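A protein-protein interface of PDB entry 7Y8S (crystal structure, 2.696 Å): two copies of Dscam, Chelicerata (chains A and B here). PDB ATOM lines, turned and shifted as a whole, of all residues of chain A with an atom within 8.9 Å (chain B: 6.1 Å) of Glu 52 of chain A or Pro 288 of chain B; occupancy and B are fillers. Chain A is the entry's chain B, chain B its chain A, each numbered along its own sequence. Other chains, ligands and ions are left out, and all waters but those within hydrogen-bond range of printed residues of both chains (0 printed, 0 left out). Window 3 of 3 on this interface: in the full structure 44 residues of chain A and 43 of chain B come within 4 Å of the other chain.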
ATOM      1  N   TYR A  36      17.592   3.131   7.946  1.00  0.00           N
ATOM      2  CA  TYR A  36      18.103   1.804   7.627  1.00  0.00           C
ATOM      3  C   TYR A  36      17.406   0.784   8.520  1.00  0.00           C
ATOM      4  O   TYR A  36      17.359   0.951   9.743  1.00  0.00           O
ATOM      5  CB  TYR A  36      19.621   1.738   7.810  1.00  0.00           C
ATOM      6  CG  TYR A  36      20.401   2.477   6.743  1.00  0.00           C
ATOM      7  CD1 TYR A  36      20.382   2.051   5.423  1.00  0.00           C
ATOM      8  CD2 TYR A  36      21.161   3.598   7.057  1.00  0.00           C
ATOM      9  CE1 TYR A  36      21.096   2.722   4.443  1.00  0.00           C
ATOM     10  CE2 TYR A  36      21.877   4.277   6.082  1.00  0.00           C
ATOM     11  CZ  TYR A  36      21.842   3.834   4.777  1.00  0.00           C
ATOM     12  OH  TYR A  36      22.554   4.504   3.805  1.00  0.00           O
ATOM     13  N   PHE A  37      16.863  -0.267   7.905  1.00  0.00           N
ATOM     14  CA  PHE A  37      16.051  -1.271   8.587  1.00  0.00           C
ATOM     15  C   PHE A  37      16.802  -2.594   8.551  1.00  0.00           C
ATOM     16  O   PHE A  37      17.115  -3.101   7.469  1.00  0.00           O
ATOM     17  CB  PHE A  37      14.681  -1.397   7.911  1.00  0.00           C
ATOM     18  CG  PHE A  37      13.604  -1.986   8.784  1.00  0.00           C
ATOM     19  CD1 PHE A  37      13.423  -1.550  10.088  1.00  0.00           C
ATOM     20  CD2 PHE A  37      12.748  -2.957   8.285  1.00  0.00           C
ATOM     21  CE1 PHE A  37      12.419  -2.091  10.884  1.00  0.00           C
ATOM     22  CE2 PHE A  37      11.743  -3.499   9.072  1.00  0.00           C
ATOM     23  CZ  PHE A  37      11.580  -3.065  10.374  1.00  0.00           C
ATOM     24  N   VAL A  38      17.096  -3.150   9.725  1.00  0.00           N
ATOM     25  CA  VAL A  38      17.915  -4.352   9.843  1.00  0.00           C
ATOM     26  C   VAL A  38      17.043  -5.483  10.368  1.00  0.00           C
ATOM     27  O   VAL A  38      16.615  -5.463  11.528  1.00  0.00           O
ATOM     28  CB  VAL A  38      19.127  -4.133  10.756  1.00  0.00           C
ATOM     29  CG1 VAL A  38      19.928  -5.413  10.873  1.00  0.00           C
ATOM     30  CG2 VAL A  38      19.994  -2.995  10.233  1.00  0.00           C
ATOM     31  N   GLN A  39      16.776  -6.469   9.520  1.00  0.00           N
ATOM     32  CA  GLN A  39      16.108  -7.694   9.934  1.00  0.00           C
ATOM     33  C   GLN A  39      17.133  -8.818  10.055  1.00  0.00           C
ATOM     34  O   GLN A  39      18.119  -8.864   9.313  1.00  0.00           O
ATOM     35  CB  GLN A  39      15.014  -8.089   8.940  1.00  0.00           C
ATOM     36  CG  GLN A  39      14.010  -7.000   8.629  1.00  0.00           C
ATOM     37  CD  GLN A  39      13.083  -7.381   7.489  1.00  0.00           C
ATOM     38  OE1 GLN A  39      13.521  -7.530   6.346  1.00  0.00           O
ATOM     39  NE2 GLN A  39      11.797  -7.550   7.795  1.00  0.00           N
ATOM     40  N   TYR A  40      16.901  -9.716  11.013  1.00  0.00           N
ATOM     41  CA  TYR A  40      17.769 -10.875  11.184  1.00  0.00           C
ATOM     42  C   TYR A  40      17.008 -11.963  11.926  1.00  0.00           C
ATOM     43  O   TYR A  40      16.152 -11.678  12.766  1.00  0.00           O
ATOM     44  CB  TYR A  40      19.071 -10.522  11.918  1.00  0.00           C
ATOM     45  CG  TYR A  40      18.903 -10.036  13.341  1.00  0.00           C
ATOM     46  CD1 TYR A  40      18.595  -8.708  13.613  1.00  0.00           C
ATOM     47  CD2 TYR A  40      19.066 -10.903  14.415  1.00  0.00           C
ATOM     48  CE1 TYR A  40      18.446  -8.261  14.918  1.00  0.00           C
ATOM     49  CE2 TYR A  40      18.919 -10.465  15.720  1.00  0.00           C
ATOM     50  CZ  TYR A  40      18.608  -9.145  15.966  1.00  0.00           C
ATOM     51  OH  TYR A  40      18.463  -8.707  17.264  1.00  0.00           O
ATOM     52  N   TRP A  41      17.328 -13.214  11.596  1.00  0.00           N
ATOM     53  CA  TRP A  41      16.629 -14.366  12.152  1.00  0.00           C
ATOM     54  C   TRP A  41      17.546 -15.580  12.080  1.00  0.00           C
ATOM     55  O   TRP A  41      18.530 -15.595  11.334  1.00  0.00           O
ATOM     56  CB  TRP A  41      15.312 -14.634  11.410  1.00  0.00           C
ATOM     57  CG  TRP A  41      15.494 -14.951   9.945  1.00  0.00           C
ATOM     58  CD1 TRP A  41      15.395 -16.176   9.359  1.00  0.00           C
ATOM     59  CD2 TRP A  41      15.812 -14.028   8.890  1.00  0.00           C
ATOM     60  NE1 TRP A  41      15.631 -16.079   8.010  1.00  0.00           N
ATOM     61  CE2 TRP A  41      15.889 -14.772   7.695  1.00  0.00           C
ATOM     62  CE3 TRP A  41      16.027 -12.647   8.839  1.00  0.00           C
ATOM     63  CZ2 TRP A  41      16.179 -14.182   6.463  1.00  0.00           C
ATOM     64  CZ3 TRP A  41      16.321 -12.061   7.616  1.00  0.00           C
ATOM     65  CH2 TRP A  41      16.393 -12.830   6.445  1.00  0.00           C
ATOM     66  N   GLN A  48      10.701 -19.129  12.734  1.00  0.00           N
ATOM     67  CA  GLN A  48      11.620 -18.407  13.604  1.00  0.00           C
ATOM     68  C   GLN A  48      11.104 -16.996  13.863  1.00  0.00           C
ATOM     69  O   GLN A  48      10.190 -16.504  13.194  1.00  0.00           O
ATOM     70  CB  GLN A  48      13.032 -18.349  13.000  1.00  0.00           C
ATOM     71  CG  GLN A  48      13.611 -19.712  12.667  1.00  0.00           C
ATOM     72  CD  GLN A  48      13.692 -20.620  13.878  1.00  0.00           C
ATOM     73  OE1 GLN A  48      14.195 -20.226  14.931  1.00  0.00           O
ATOM     74  NE2 GLN A  48      13.190 -21.844  13.735  1.00  0.00           N
ATOM     75  N   MET A  49      11.717 -16.340  14.844  1.00  0.00           N
ATOM     76  CA  MET A  49      11.369 -14.974  15.209  1.00  0.00           C
ATOM     77  C   MET A  49      12.097 -13.996  14.297  1.00  0.00           C
ATOM     78  O   MET A  49      13.319 -14.081  14.136  1.00  0.00           O
ATOM     79  CB  MET A  49      11.731 -14.704  16.670  1.00  0.00           C
ATOM     80  CG  MET A  49      10.943 -15.548  17.673  1.00  0.00           C
ATOM     81  SD  MET A  49      11.734 -15.680  19.297  1.00  0.00           S
ATOM     82  CE  MET A  49      11.969 -13.947  19.694  1.00  0.00           C
ATOM     83  N   LEU A  50      11.349 -13.066  13.706  1.00  0.00           N
ATOM     84  CA  LEU A  50      11.920 -12.066  12.804  1.00  0.00           C
ATOM     85  C   LEU A  50      12.263 -10.827  13.623  1.00  0.00           C
ATOM     86  O   LEU A  50      11.396 -10.008  13.931  1.00  0.00           O
ATOM     87  CB  LEU A  50      10.952 -11.745  11.672  1.00  0.00           C
ATOM     88  CG  LEU A  50      11.445 -10.747  10.622  1.00  0.00           C
ATOM     89  CD1 LEU A  50      12.858 -11.082  10.178  1.00  0.00           C
ATOM     90  CD2 LEU A  50      10.499 -10.700   9.426  1.00  0.00           C
ATOM     91  N   GLN A  51      13.538 -10.690  13.975  1.00  0.00           N
ATOM     92  CA  GLN A  51      14.006  -9.577  14.786  1.00  0.00           C
ATOM     93  C   GLN A  51      14.323  -8.378  13.903  1.00  0.00           C
ATOM     94  O   GLN A  51      14.898  -8.524  12.821  1.00  0.00           O
ATOM     95  CB  GLN A  51      15.245  -9.986  15.581  1.00  0.00           C
ATOM     96  CG  GLN A  51      14.987 -11.132  16.538  1.00  0.00           C
ATOM     97  CD  GLN A  51      15.066 -10.708  17.986  1.00  0.00           C
ATOM     98  OE1 GLN A  51      14.399  -9.761  18.403  1.00  0.00           O
ATOM     99  NE2 GLN A  51      15.889 -11.407  18.766  1.00  0.00           N
ATOM    100  N   GLU A  52      13.944  -7.191  14.375  1.00  0.00           N
ATOM    101  CA  GLU A  52      14.061  -5.972  13.588  1.00  0.00           C
ATOM    102  C   GLU A  52      14.620  -4.853  14.452  1.00  0.00           C
ATOM    103  O   GLU A  52      14.402  -4.812  15.665  1.00  0.00           O
ATOM    104  CB  GLU A  52      12.706  -5.561  12.997  1.00  0.00           C
ATOM    105  CG  GLU A  52      12.060  -6.648  12.148  1.00  0.00           C
ATOM    106  CD  GLU A  52      10.800  -6.179  11.453  1.00  0.00           C
ATOM    107  OE1 GLU A  52       9.945  -5.570  12.128  1.00  0.00           O
ATOM    108  OE2 GLU A  52      10.666  -6.421  10.234  1.00  0.00           O
ATOM    109  N   GLU A  53      15.333  -3.932  13.809  1.00  0.00           N
ATOM    110  CA  GLU A  53      16.019  -2.862  14.521  1.00  0.00           C
ATOM    111  C   GLU A  53      16.315  -1.740  13.539  1.00  0.00           C
ATOM    112  O   GLU A  53      16.783  -2.000  12.426  1.00  0.00           O
ATOM    113  CB  GLU A  53      17.312  -3.375  15.165  1.00  0.00           C
ATOM    114  CG  GLU A  53      18.026  -2.354  16.027  1.00  0.00           C
ATOM    115  CD  GLU A  53      18.910  -3.007  17.069  1.00  0.00           C
ATOM    116  OE1 GLU A  53      18.356  -3.600  18.019  1.00  0.00           O
ATOM    117  OE2 GLU A  53      20.152  -2.929  16.936  1.00  0.00           O
ATOM    118  N   GLU A  54      16.050  -0.503  13.952  1.00  0.00           N
ATOM    119  CA  GLU A  54      16.221   0.664  13.100  1.00  0.00           C
ATOM    120  C   GLU A  54      17.537   1.376  13.397  1.00  0.00           C
ATOM    121  O   GLU A  54      18.099   1.278  14.490  1.00  0.00           O
ATOM    122  CB  GLU A  54      15.053   1.637  13.274  1.00  0.00           C
ATOM    123  CG  GLU A  54      13.844   1.312  12.421  1.00  0.00           C
ATOM    124  CD  GLU A  54      12.699   2.273  12.657  1.00  0.00           C
ATOM    125  OE1 GLU A  54      11.561   1.802  12.878  1.00  0.00           O
ATOM    126  OE2 GLU A  54      12.939   3.500  12.626  1.00  0.00           O
ATOM    127  N   VAL A  55      18.010   2.109  12.395  1.00  0.00           N
ATOM    128  CA  VAL A  55      19.247   2.885  12.454  1.00  0.00           C
ATOM    129  C   VAL A  55      19.047   4.128  11.589  1.00  0.00           C
ATOM    130  O   VAL A  55      18.458   4.049  10.507  1.00  0.00           O
ATOM    131  CB  VAL A  55      20.455   2.048  11.970  1.00  0.00           C
ATOM    132  CG1 VAL A  55      21.664   2.919  11.749  1.00  0.00           C
ATOM    133  CG2 VAL A  55      20.787   0.933  12.953  1.00  0.00           C
ATOM    134  N   ILE A  64      24.693  -5.763  16.356  1.00  0.00           N
ATOM    135  CA  ILE A  64      23.572  -6.573  16.821  1.00  0.00           C
ATOM    136  C   ILE A  64      24.016  -7.357  18.048  1.00  0.00           C
ATOM    137  O   ILE A  64      25.104  -7.945  18.056  1.00  0.00           O
ATOM    138  CB  ILE A  64      23.076  -7.516  15.712  1.00  0.00           C
ATOM    139  CG1 ILE A  64      22.649  -6.716  14.478  1.00  0.00           C
ATOM    140  CG2 ILE A  64      21.941  -8.379  16.225  1.00  0.00           C
ATOM    141  CD1 ILE A  64      21.499  -5.760  14.728  1.00  0.00           C
ATOM    142  N   THR A  76      19.177  -9.031   6.758  1.00  0.00           N
ATOM    143  CA  THR A  76      18.965  -8.116   5.648  1.00  0.00           C
ATOM    144  C   THR A  76      18.940  -6.677   6.146  1.00  0.00           C
ATOM    145  O   THR A  76      18.366  -6.378   7.200  1.00  0.00           O
ATOM    146  CB  THR A  76      17.662  -8.433   4.896  1.00  0.00           C
ATOM    147  OG1 THR A  76      17.327  -7.339   4.029  1.00  0.00           O
ATOM    148  CG2 THR A  76      16.531  -8.693   5.862  1.00  0.00           C
ATOM    149  N   ILE A  78      17.724  -2.882   4.893  1.00  0.00           N
ATOM    150  CA  ILE A  78      16.855  -2.178   3.956  1.00  0.00           C
ATOM    151  C   ILE A  78      17.059  -0.679   4.129  1.00  0.00           C
ATOM    152  O   ILE A  78      17.030  -0.171   5.255  1.00  0.00           O
ATOM    153  CB  ILE A  78      15.374  -2.540   4.167  1.00  0.00           C
ATOM    154  CG1 ILE A  78      15.188  -4.055   4.253  1.00  0.00           C
ATOM    155  CG2 ILE A  78      14.528  -1.954   3.055  1.00  0.00           C
ATOM    156  CD1 ILE A  78      13.768  -4.471   4.580  1.00  0.00           C
ATOM    157  N   GLU A  80      15.204   2.453   3.608  1.00  0.00           N
ATOM    158  CA  GLU A  80      13.860   2.941   3.316  1.00  0.00           C
ATOM    159  C   GLU A  80      13.921   4.303   2.631  1.00  0.00           C
ATOM    160  O   GLU A  80      14.921   5.021   2.713  1.00  0.00           O
ATOM    161  CB  GLU A  80      13.040   3.072   4.588  1.00  0.00           C
ATOM    162  CG  GLU A  80      12.830   1.779   5.316  1.00  0.00           C
ATOM    163  CD  GLU A  80      11.559   1.735   6.111  1.00  0.00           C
ATOM    164  OE1 GLU A  80      10.517   2.194   5.603  1.00  0.00           O
ATOM    165  OE2 GLU A  80      11.617   1.230   7.255  1.00  0.00           O
ATOM    166  N   GLU B 111       6.519 -14.222  21.104  1.00  0.00           N
ATOM    167  CA  GLU B 111       5.999 -13.174  20.245  1.00  0.00           C
ATOM    168  C   GLU B 111       5.134 -12.246  21.074  1.00  0.00           C
ATOM    169  O   GLU B 111       4.344 -12.699  21.911  1.00  0.00           O
ATOM    170  CB  GLU B 111       5.210 -13.723  19.059  1.00  0.00           C
ATOM    171  CG  GLU B 111       5.938 -13.516  17.734  1.00  0.00           C
ATOM    172  CD  GLU B 111       5.023 -13.528  16.530  1.00  0.00           C
ATOM    173  OE1 GLU B 111       3.923 -14.113  16.614  1.00  0.00           O
ATOM    174  OE2 GLU B 111       5.423 -12.970  15.488  1.00  0.00           O
ATOM    175  N   PRO B 208       0.775  -8.622  14.411  1.00  0.00           N
ATOM    176  CA  PRO B 208       1.399  -9.511  13.424  1.00  0.00           C
ATOM    177  C   PRO B 208       0.535 -10.726  13.146  1.00  0.00           C
ATOM    178  O   PRO B 208       0.108 -11.424  14.080  1.00  0.00           O
ATOM    179  CB  PRO B 208       2.721  -9.909  14.097  1.00  0.00           C
ATOM    180  CG  PRO B 208       2.481  -9.707  15.560  1.00  0.00           C
ATOM    181  CD  PRO B 208       1.573  -8.519  15.646  1.00  0.00           C
ATOM    182  N   PRO B 209       0.271 -11.018  11.872  1.00  0.00           N
ATOM    183  CA  PRO B 209      -0.537 -12.192  11.537  1.00  0.00           C
ATOM    184  C   PRO B 209       0.148 -13.471  12.002  1.00  0.00           C
ATOM    185  O   PRO B 209       1.360 -13.518  12.224  1.00  0.00           O
ATOM    186  CB  PRO B 209      -0.629 -12.138  10.005  1.00  0.00           C
ATOM    187  CG  PRO B 209      -0.195 -10.740   9.618  1.00  0.00           C
ATOM    188  CD  PRO B 209       0.777 -10.326  10.675  1.00  0.00           C
ATOM    189  N   TYR B 276       7.150 -14.706   5.170  1.00  0.00           N
ATOM    190  CA  TYR B 276       6.466 -14.044   6.273  1.00  0.00           C
ATOM    191  C   TYR B 276       5.499 -13.018   5.706  1.00  0.00           C
ATOM    192  O   TYR B 276       5.612 -12.600   4.550  1.00  0.00           O
ATOM    193  CB  TYR B 276       7.444 -13.396   7.264  1.00  0.00           C
ATOM    194  CG  TYR B 276       8.071 -12.104   6.814  1.00  0.00           C
ATOM    195  CD1 TYR B 276       9.245 -12.103   6.078  1.00  0.00           C
ATOM    196  CD2 TYR B 276       7.506 -10.878   7.150  1.00  0.00           C
ATOM    197  CE1 TYR B 276       9.835 -10.919   5.675  1.00  0.00           C
ATOM    198  CE2 TYR B 276       8.089  -9.686   6.748  1.00  0.00           C
ATOM    199  CZ  TYR B 276       9.253  -9.716   6.011  1.00  0.00           C
ATOM    200  OH  TYR B 276       9.847  -8.543   5.609  1.00  0.00           O
ATOM    201  N   VAL B 277       4.539 -12.620   6.541  1.00  0.00           N
ATOM    202  CA  VAL B 277       3.418 -11.782   6.130  1.00  0.00           C
ATOM    203  C   VAL B 277       3.336 -10.567   7.045  1.00  0.00           C
ATOM    204  O   VAL B 277       3.456 -10.691   8.269  1.00  0.00           O
ATOM    205  CB  VAL B 277       2.091 -12.567   6.165  1.00  0.00           C
ATOM    206  CG1 VAL B 277       0.932 -11.676   5.781  1.00  0.00           C
ATOM    207  CG2 VAL B 277       2.168 -13.769   5.238  1.00  0.00           C
ATOM    208  N   THR B 278       3.128  -9.395   6.450  1.00  0.00           N
ATOM    209  CA  THR B 278       2.858  -8.181   7.202  1.00  0.00           C
ATOM    210  C   THR B 278       1.475  -7.663   6.843  1.00  0.00           C
ATOM    211  O   THR B 278       0.991  -7.855   5.723  1.00  0.00           O
ATOM    212  CB  THR B 278       3.889  -7.078   6.930  1.00  0.00           C
ATOM    213  OG1 THR B 278       3.996  -6.858   5.521  1.00  0.00           O
ATOM    214  CG2 THR B 278       5.250  -7.451   7.496  1.00  0.00           C
ATOM    215  N   ARG B 285       2.457   0.043   8.301  1.00  0.00           N
ATOM    216  CA  ARG B 285       2.743  -1.386   8.237  1.00  0.00           C
ATOM    217  C   ARG B 285       2.990  -1.945   9.631  1.00  0.00           C
ATOM    218  O   ARG B 285       3.796  -1.404  10.396  1.00  0.00           O
ATOM    219  CB  ARG B 285       3.953  -1.655   7.342  1.00  0.00           C
ATOM    220  CG  ARG B 285       4.190  -3.127   7.036  1.00  0.00           C
ATOM    221  CD  ARG B 285       5.551  -3.348   6.377  1.00  0.00           C
ATOM    222  NE  ARG B 285       6.634  -2.607   7.029  1.00  0.00           N
ATOM    223  CZ  ARG B 285       7.080  -2.833   8.264  1.00  0.00           C
ATOM    224  NH1 ARG B 285       6.549  -3.792   9.015  1.00  0.00           N
ATOM    225  NH2 ARG B 285       8.068  -2.097   8.755  1.00  0.00           N
ATOM    226  N   GLY B 286       2.296  -3.035   9.952  1.00  0.00           N
ATOM    227  CA  GLY B 286       2.439  -3.664  11.245  1.00  0.00           C
ATOM    228  C   GLY B 286       3.616  -4.620  11.312  1.00  0.00           C
ATOM    229  O   GLY B 286       4.214  -4.992  10.302  1.00  0.00           O
ATOM    230  N   ASP B 287       3.938  -5.023  12.541  1.00  0.00           N
ATOM    231  CA  ASP B 287       5.060  -5.919  12.772  1.00  0.00           C
ATOM    232  C   ASP B 287       4.864  -7.239  12.023  1.00  0.00           C
ATOM    233  O   ASP B 287       3.734  -7.650  11.748  1.00  0.00           O
ATOM    234  CB  ASP B 287       5.232  -6.170  14.268  1.00  0.00           C
ATOM    235  CG  ASP B 287       6.112  -5.127  14.931  1.00  0.00           C
ATOM    236  OD1 ASP B 287       6.424  -4.108  14.271  1.00  0.00           O
ATOM    237  OD2 ASP B 287       6.495  -5.330  16.106  1.00  0.00           O
ATOM    238  N   PRO B 288       5.951  -7.921  11.675  1.00  0.00           N
ATOM    239  CA  PRO B 288       5.846  -9.092  10.802  1.00  0.00           C
ATOM    240  C   PRO B 288       5.417 -10.354  11.541  1.00  0.00           C
ATOM    241  O   PRO B 288       5.393 -10.420  12.770  1.00  0.00           O
ATOM    242  CB  PRO B 288       7.273  -9.244  10.267  1.00  0.00           C
ATOM    243  CG  PRO B 288       8.125  -8.718  11.374  1.00  0.00           C
ATOM    244  CD  PRO B 288       7.356  -7.543  11.918  1.00  0.00           C
ATOM    245  N   SER B 289       5.097 -11.377  10.744  1.00  0.00           N
ATOM    246  CA  SER B 289       4.809 -12.724  11.223  1.00  0.00           C
ATOM    247  C   SER B 289       6.049 -13.329  11.872  1.00  0.00           C
ATOM    248  O   SER B 289       7.103 -12.689  11.927  1.00  0.00           O
ATOM    249  CB  SER B 289       4.371 -13.619  10.060  1.00  0.00           C
ATOM    250  OG  SER B 289       3.136 -13.209   9.502  1.00  0.00           O
ATOM    251  N   GLY B 290       5.932 -14.546  12.395  1.00  0.00           N
ATOM    252  CA  GLY B 290       7.090 -15.415  12.425  1.00  0.00           C
ATOM    253  C   GLY B 290       7.542 -15.706  11.007  1.00  0.00           C
ATOM    254  O   GLY B 290       6.749 -15.674  10.063  1.00  0.00           O
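Of the 12 printed residues of chain B, 5 touch a printed residue of chain A.
Printed residues of chain B that touch a printed residue of chain A: Tyr 276, Arg 285, Pro 288, Ser 289 and Gly 290.
Hydrophobic or aromatic side chains of chain A that line the printed part of chain B: Phe 37 and Leu 50.
Among the printed residues, 7 pairs touch across the chains.
No position is printed for both chains.
Of the 7 pairs that touch across the chains among the printed residues, none has its exchanged pair printed and touching as well.
Among the printed residues, merely in contact across the chains: Phe 37 of chain A with Arg 285 of chain B, Gln 48 of chain A with Gly 290 of chain B, Leu 50 of chain A with Tyr 276 of chain B, Leu 50 of chain A with Pro 288 of chain B, Leu 50 of chain A with Ser 289 of chain B and Glu 52 of chain A with Pro 288 of chain B.
Of the printed residues of chain B, Gln 48 of chain A touches Gly 290 (3.4 Å).
Of chain B, only Pro 288 comes within 4 Å of Glu 52 of chain A.
Val 55 of chain A touches none of the printed residues of chain B.
Of the printed residues of chain A, Tyr 276 of chain B touches Gln 39 and Leu 50.
Val 277 of chain B touches none of the printed residues of chain A.
Printed residues of chain A within 4 Å of Arg 285 of chain B: Phe 37 (3.9 Å).
Of the printed residues of chain A, Pro 288 of chain B touches Leu 50 and Glu 52.
Printed residues of chain A within 4 Å of Gly 290 of chain B: Gln 48 (3.4 Å).
The nearest residue of chain A that does not touch Pro 288 of chain B is Gln 39 of chain A (5.3 Å).
The nearest printed residue of chain A that does not touch Tyr 276 of chain B is Glu 52 of chain A (5.2 Å).
OH of Tyr 276 of chain B sits at hydrogen-bond distance from NE2 of Gln 39 of chain A (3.1 Å).
The backbone carbonyl oxygen (O) of Pro 209 of chain B lies within hydrogen-bond range of the side-chain hydroxyl (OG) of Ser 289 of chain B (3.3 Å).
O of Val 277 of chain B sits at hydrogen-bond distance from OG of Ser 289 of chain B (2.8 Å).
The backbone NH of Ile 78 of chain A sits at hydrogen-bond distance from the backbone carbonyl oxygen of Phe 37 of chain A, at 2.7 Å.
The side-chain amide nitrogen (NE2) of Gln 39 of chain A is in hydrogen-bond range of the side-chain carboxylate (OE2) of Glu 52 of chain A, at 2.9 Å.
The backbone carbonyl oxygen of Gln 39 of chain A is in hydrogen-bond range of the backbone NH of Thr 76 of chain A, at 2.8 Å.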
